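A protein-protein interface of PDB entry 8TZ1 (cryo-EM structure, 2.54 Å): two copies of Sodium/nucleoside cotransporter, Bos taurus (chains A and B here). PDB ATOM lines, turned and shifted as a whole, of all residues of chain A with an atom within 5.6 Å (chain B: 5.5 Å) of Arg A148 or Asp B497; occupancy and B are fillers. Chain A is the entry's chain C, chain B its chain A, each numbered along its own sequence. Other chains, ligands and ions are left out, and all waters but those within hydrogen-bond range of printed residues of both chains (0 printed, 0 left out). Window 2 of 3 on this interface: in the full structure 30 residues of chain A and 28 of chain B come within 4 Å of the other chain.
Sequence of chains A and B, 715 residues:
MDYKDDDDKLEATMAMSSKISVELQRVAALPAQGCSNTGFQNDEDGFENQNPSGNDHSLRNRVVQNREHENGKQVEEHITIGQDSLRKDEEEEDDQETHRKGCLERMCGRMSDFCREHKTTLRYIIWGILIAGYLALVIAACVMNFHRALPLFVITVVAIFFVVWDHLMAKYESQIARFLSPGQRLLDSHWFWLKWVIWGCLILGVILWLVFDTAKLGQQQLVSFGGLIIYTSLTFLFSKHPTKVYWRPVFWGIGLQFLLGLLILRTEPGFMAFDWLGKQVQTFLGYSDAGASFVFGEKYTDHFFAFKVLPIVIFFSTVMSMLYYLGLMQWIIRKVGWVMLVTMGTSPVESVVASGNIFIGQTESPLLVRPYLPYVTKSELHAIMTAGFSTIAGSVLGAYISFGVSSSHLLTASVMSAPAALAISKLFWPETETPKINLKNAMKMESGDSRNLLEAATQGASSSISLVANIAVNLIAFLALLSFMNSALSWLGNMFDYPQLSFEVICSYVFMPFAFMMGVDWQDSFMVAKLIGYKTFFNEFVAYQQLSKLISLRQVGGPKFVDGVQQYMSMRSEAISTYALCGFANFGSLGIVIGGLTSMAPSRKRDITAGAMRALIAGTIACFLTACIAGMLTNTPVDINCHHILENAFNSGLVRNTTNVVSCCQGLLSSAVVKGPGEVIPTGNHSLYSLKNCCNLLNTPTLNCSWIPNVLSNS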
ATOM      1  N   MET A 144       7.091 -19.550   1.565  1.00  0.00           N
ATOM      2  CA  MET A 144       6.021 -18.682   1.083  1.00  0.00           C
ATOM      3  C   MET A 144       4.774 -18.821   1.944  1.00  0.00           C
ATOM      4  O   MET A 144       4.122 -17.822   2.274  1.00  0.00           O
ATOM      5  CB  MET A 144       5.704 -19.005  -0.378  1.00  0.00           C
ATOM      6  CG  MET A 144       6.866 -18.765  -1.328  1.00  0.00           C
ATOM      7  SD  MET A 144       6.421 -18.976  -3.062  1.00  0.00           S
ATOM      8  CE  MET A 144       5.295 -17.601  -3.294  1.00  0.00           C
ATOM      9  N   ASN A 145       4.424 -20.049   2.316  1.00  0.00           N
ATOM     10  CA  ASN A 145       3.290 -20.297   3.197  1.00  0.00           C
ATOM     11  C   ASN A 145       3.429 -21.704   3.753  1.00  0.00           C
ATOM     12  O   ASN A 145       3.639 -22.652   2.992  1.00  0.00           O
ATOM     13  CB  ASN A 145       1.962 -20.130   2.452  1.00  0.00           C
ATOM     14  CG  ASN A 145       0.759 -20.235   3.369  1.00  0.00           C
ATOM     15  OD1 ASN A 145       0.807 -20.897   4.405  1.00  0.00           O
ATOM     16  ND2 ASN A 145      -0.330 -19.582   2.988  1.00  0.00           N
ATOM     17  N   PHE A 146       3.306 -21.834   5.072  1.00  0.00           N
ATOM     18  CA  PHE A 146       3.543 -23.110   5.735  1.00  0.00           C
ATOM     19  C   PHE A 146       2.269 -23.942   5.850  1.00  0.00           C
ATOM     20  O   PHE A 146       2.274 -25.133   5.525  1.00  0.00           O
ATOM     21  CB  PHE A 146       4.141 -22.872   7.122  1.00  0.00           C
ATOM     22  CG  PHE A 146       4.733 -24.103   7.740  1.00  0.00           C
ATOM     23  CD1 PHE A 146       6.059 -24.432   7.522  1.00  0.00           C
ATOM     24  CD2 PHE A 146       3.963 -24.935   8.534  1.00  0.00           C
ATOM     25  CE1 PHE A 146       6.606 -25.565   8.086  1.00  0.00           C
ATOM     26  CE2 PHE A 146       4.506 -26.069   9.100  1.00  0.00           C
ATOM     27  CZ  PHE A 146       5.828 -26.384   8.875  1.00  0.00           C
ATOM     28  N   HIS A 147       1.177 -23.332   6.312  1.00  0.00           N
ATOM     29  CA  HIS A 147      -0.072 -24.073   6.454  1.00  0.00           C
ATOM     30  C   HIS A 147      -0.534 -24.648   5.123  1.00  0.00           C
ATOM     31  O   HIS A 147      -1.136 -25.727   5.086  1.00  0.00           O
ATOM     32  CB  HIS A 147      -1.154 -23.167   7.042  1.00  0.00           C
ATOM     33  CG  HIS A 147      -2.477 -23.842   7.214  1.00  0.00           C
ATOM     34  ND1 HIS A 147      -2.664 -24.914   8.060  1.00  0.00           N
ATOM     35  CD2 HIS A 147      -3.684 -23.597   6.648  1.00  0.00           C
ATOM     36  CE1 HIS A 147      -3.926 -25.300   8.008  1.00  0.00           C
ATOM     37  NE2 HIS A 147      -4.567 -24.517   7.158  1.00  0.00           N
ATOM     38  N   ARG A 148      -0.265 -23.943   4.023  1.00  0.00           N
ATOM     39  CA  ARG A 148      -0.672 -24.420   2.707  1.00  0.00           C
ATOM     40  C   ARG A 148       0.228 -25.538   2.196  1.00  0.00           C
ATOM     41  O   ARG A 148      -0.230 -26.394   1.432  1.00  0.00           O
ATOM     42  CB  ARG A 148      -0.675 -23.255   1.718  1.00  0.00           C
ATOM     43  CG  ARG A 148      -1.232 -23.595   0.351  1.00  0.00           C
ATOM     44  CD  ARG A 148      -1.357 -22.349  -0.506  1.00  0.00           C
ATOM     45  NE  ARG A 148      -0.082 -21.657  -0.650  1.00  0.00           N
ATOM     46  CZ  ARG A 148       0.062 -20.458  -1.197  1.00  0.00           C
ATOM     47  NH1 ARG A 148      -0.975 -19.778  -1.658  1.00  0.00           N
ATOM     48  NH2 ARG A 148       1.277 -19.926  -1.282  1.00  0.00           N
ATOM     49  N   ALA A 149       1.497 -25.550   2.604  1.00  0.00           N
ATOM     50  CA  ALA A 149       2.469 -26.532   2.143  1.00  0.00           C
ATOM     51  C   ALA A 149       2.705 -27.647   3.154  1.00  0.00           C
ATOM     52  O   ALA A 149       3.661 -28.414   2.999  1.00  0.00           O
ATOM     53  CB  ALA A 149       3.794 -25.844   1.821  1.00  0.00           C
ATOM     54  N   LEU A 150       1.864 -27.754   4.178  1.00  0.00           N
ATOM     55  CA  LEU A 150       2.101 -28.742   5.228  1.00  0.00           C
ATOM     56  C   LEU A 150       2.129 -30.168   4.700  1.00  0.00           C
ATOM     57  O   LEU A 150       3.097 -30.893   4.992  1.00  0.00           O
ATOM     58  CB  LEU A 150       1.040 -28.582   6.322  1.00  0.00           C
ATOM     59  CG  LEU A 150       1.263 -29.399   7.595  1.00  0.00           C
ATOM     60  CD1 LEU A 150       2.457 -28.865   8.371  1.00  0.00           C
ATOM     61  CD2 LEU A 150       0.012 -29.386   8.453  1.00  0.00           C
ATOM     62  N   PRO A 151       1.138 -30.643   3.936  1.00  0.00           N
ATOM     63  CA  PRO A 151       1.172 -32.053   3.509  1.00  0.00           C
ATOM     64  C   PRO A 151       2.410 -32.414   2.708  1.00  0.00           C
ATOM     65  O   PRO A 151       2.933 -33.525   2.854  1.00  0.00           O
ATOM     66  CB  PRO A 151      -0.114 -32.202   2.683  1.00  0.00           C
ATOM     67  CG  PRO A 151      -0.519 -30.820   2.325  1.00  0.00           C
ATOM     68  CD  PRO A 151      -0.066 -29.952   3.447  1.00  0.00           C
ATOM     69  N   GLY B 493       1.478 -26.596  -7.481  1.00  0.00           N
ATOM     70  CA  GLY B 493       1.729 -25.245  -7.945  1.00  0.00           C
ATOM     71  C   GLY B 493       1.067 -24.173  -7.109  1.00  0.00           C
ATOM     72  O   GLY B 493       1.504 -23.018  -7.145  1.00  0.00           O
ATOM     73  N   ASN B 494       0.025 -24.525  -6.356  1.00  0.00           N
ATOM     74  CA  ASN B 494      -0.654 -23.543  -5.522  1.00  0.00           C
ATOM     75  C   ASN B 494       0.216 -23.077  -4.364  1.00  0.00           C
ATOM     76  O   ASN B 494      -0.007 -21.980  -3.842  1.00  0.00           O
ATOM     77  CB  ASN B 494      -1.963 -24.120  -4.984  1.00  0.00           C
ATOM     78  CG  ASN B 494      -2.900 -23.050  -4.461  1.00  0.00           C
ATOM     79  OD1 ASN B 494      -2.513 -21.894  -4.301  1.00  0.00           O
ATOM     80  ND2 ASN B 494      -4.140 -23.432  -4.189  1.00  0.00           N
ATOM     81  N   MET B 495       1.200 -23.878  -3.952  1.00  0.00           N
ATOM     82  CA  MET B 495       2.082 -23.458  -2.869  1.00  0.00           C
ATOM     83  C   MET B 495       2.772 -22.146  -3.214  1.00  0.00           C
ATOM     84  O   MET B 495       2.920 -21.267  -2.356  1.00  0.00           O
ATOM     85  CB  MET B 495       3.126 -24.536  -2.583  1.00  0.00           C
ATOM     86  CG  MET B 495       2.581 -25.948  -2.454  1.00  0.00           C
ATOM     87  SD  MET B 495       1.329 -26.143  -1.179  1.00  0.00           S
ATOM     88  CE  MET B 495       1.198 -27.928  -1.151  1.00  0.00           C
ATOM     89  N   PHE B 496       3.200 -21.997  -4.467  1.00  0.00           N
ATOM     90  CA  PHE B 496       3.857 -20.791  -4.941  1.00  0.00           C
ATOM     91  C   PHE B 496       2.883 -19.814  -5.589  1.00  0.00           C
ATOM     92  O   PHE B 496       3.303 -18.974  -6.393  1.00  0.00           O
ATOM     93  CB  PHE B 496       4.965 -21.157  -5.930  1.00  0.00           C
ATOM     94  CG  PHE B 496       5.837 -22.287  -5.469  1.00  0.00           C
ATOM     95  CD1 PHE B 496       6.957 -22.046  -4.694  1.00  0.00           C
ATOM     96  CD2 PHE B 496       5.536 -23.593  -5.812  1.00  0.00           C
ATOM     97  CE1 PHE B 496       7.759 -23.087  -4.270  1.00  0.00           C
ATOM     98  CE2 PHE B 496       6.335 -24.636  -5.390  1.00  0.00           C
ATOM     99  CZ  PHE B 496       7.446 -24.382  -4.620  1.00  0.00           C
ATOM    100  N   ASP B 497       1.595 -19.911  -5.262  1.00  0.00           N
ATOM    101  CA  ASP B 497       0.571 -19.025  -5.813  1.00  0.00           C
ATOM    102  C   ASP B 497       0.508 -19.114  -7.335  1.00  0.00           C
ATOM    103  O   ASP B 497       0.180 -18.136  -8.011  1.00  0.00           O
ATOM    104  CB  ASP B 497       0.804 -17.576  -5.374  1.00  0.00           C
ATOM    105  CG  ASP B 497       0.616 -17.384  -3.883  1.00  0.00           C
ATOM    106  OD1 ASP B 497      -0.277 -18.039  -3.306  1.00  0.00           O
ATOM    107  OD2 ASP B 497       1.362 -16.579  -3.286  1.00  0.00           O
ATOM    108  N   TYR B 498       0.821 -20.285  -7.886  1.00  0.00           N
ATOM    109  CA  TYR B 498       0.740 -20.541  -9.323  1.00  0.00           C
ATOM    110  C   TYR B 498      -0.033 -21.833  -9.536  1.00  0.00           C
ATOM    111  O   TYR B 498       0.558 -22.895  -9.775  1.00  0.00           O
ATOM    112  CB  TYR B 498       2.130 -20.614  -9.953  1.00  0.00           C
ATOM    113  CG  TYR B 498       2.106 -20.691 -11.461  1.00  0.00           C
ATOM    114  CD1 TYR B 498       1.480 -19.707 -12.214  1.00  0.00           C
ATOM    115  CD2 TYR B 498       2.714 -21.740 -12.132  1.00  0.00           C
ATOM    116  CE1 TYR B 498       1.454 -19.772 -13.591  1.00  0.00           C
ATOM    117  CE2 TYR B 498       2.695 -21.813 -13.509  1.00  0.00           C
ATOM    118  CZ  TYR B 498       2.064 -20.825 -14.233  1.00  0.00           C
ATOM    119  OH  TYR B 498       2.042 -20.894 -15.606  1.00  0.00           O
ATOM    120  N   PRO B 499      -1.365 -21.784  -9.458  1.00  0.00           N
ATOM    121  CA  PRO B 499      -2.173 -22.999  -9.585  1.00  0.00           C
ATOM    122  C   PRO B 499      -2.436 -23.447 -11.015  1.00  0.00           C
ATOM    123  O   PRO B 499      -3.200 -24.395 -11.211  1.00  0.00           O
ATOM    124  CB  PRO B 499      -3.485 -22.592  -8.899  1.00  0.00           C
ATOM    125  CG  PRO B 499      -3.599 -21.143  -9.176  1.00  0.00           C
ATOM    126  CD  PRO B 499      -2.194 -20.599  -9.177  1.00  0.00           C
ATOM    127  N   GLN B 500      -1.832 -22.804 -12.012  1.00  0.00           N
ATOM    128  CA  GLN B 500      -2.049 -23.153 -13.409  1.00  0.00           C
ATOM    129  C   GLN B 500      -1.012 -24.130 -13.945  1.00  0.00           C
ATOM    130  O   GLN B 500      -1.053 -24.463 -15.133  1.00  0.00           O
ATOM    131  CB  GLN B 500      -2.055 -21.893 -14.277  1.00  0.00           C
ATOM    132  CG  GLN B 500      -3.141 -20.893 -13.918  1.00  0.00           C
ATOM    133  CD  GLN B 500      -2.723 -19.932 -12.822  1.00  0.00           C
ATOM    134  OE1 GLN B 500      -1.548 -19.853 -12.463  1.00  0.00           O
ATOM    135  NE2 GLN B 500      -3.685 -19.192 -12.286  1.00  0.00           N
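Of the printed residues of chain B, Arg A148 touches Asn B494 (3.1 Å), Met B495 (2.4 Å) and Asp B497 (2.5 Å). Of the printed residues of chain A, Met B495 touches Arg A148 and Ala A149. Printed residues of chain A within 4 Å of Phe B496: Met A144. Of the printed residues of chain B, Ala A149 touches Met B495 (3.5 Å). Printed residues of chain B within 4 Å of Met A144: Phe B496. Of the printed residues of chain A, Asn B494 touches Arg A148. Tyr B498 touches none of the printed residues of chain A. The nearest residue of chain B that does not touch Arg A148 is Phe B496 (4.3 Å).
Met A144 touches Phe B496 (SD to CD1, 3.5 Å). Met B495 touches Ala A149.
Hydrophobic or aromatic side chains of chain A that line the printed part of chain B: Met A144 and Ala A149. Along chain A the printed residues that touch a printed residue of chain B span positions 144 to 149. Hydrophobic or aromatic side chains of chain B that line the printed part of chain A: Met B495 and Phe B496.
N of Arg A148 lies within hydrogen-bond range of OD1 of Asn A145, at 3.3 Å.
The backbone carbonyl oxygen (O) of Asn B494 sits close to the guanidinium group (NE) of Arg A148, at 3.2 Å. NE of Arg A148 lies close to O of Met B495 (3.5 Å). The guanidinium group (NH1) of Arg A148 is in salt-bridge range of the side-chain carboxylate (OD1) of Asp B497.
No position is printed for both chains.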
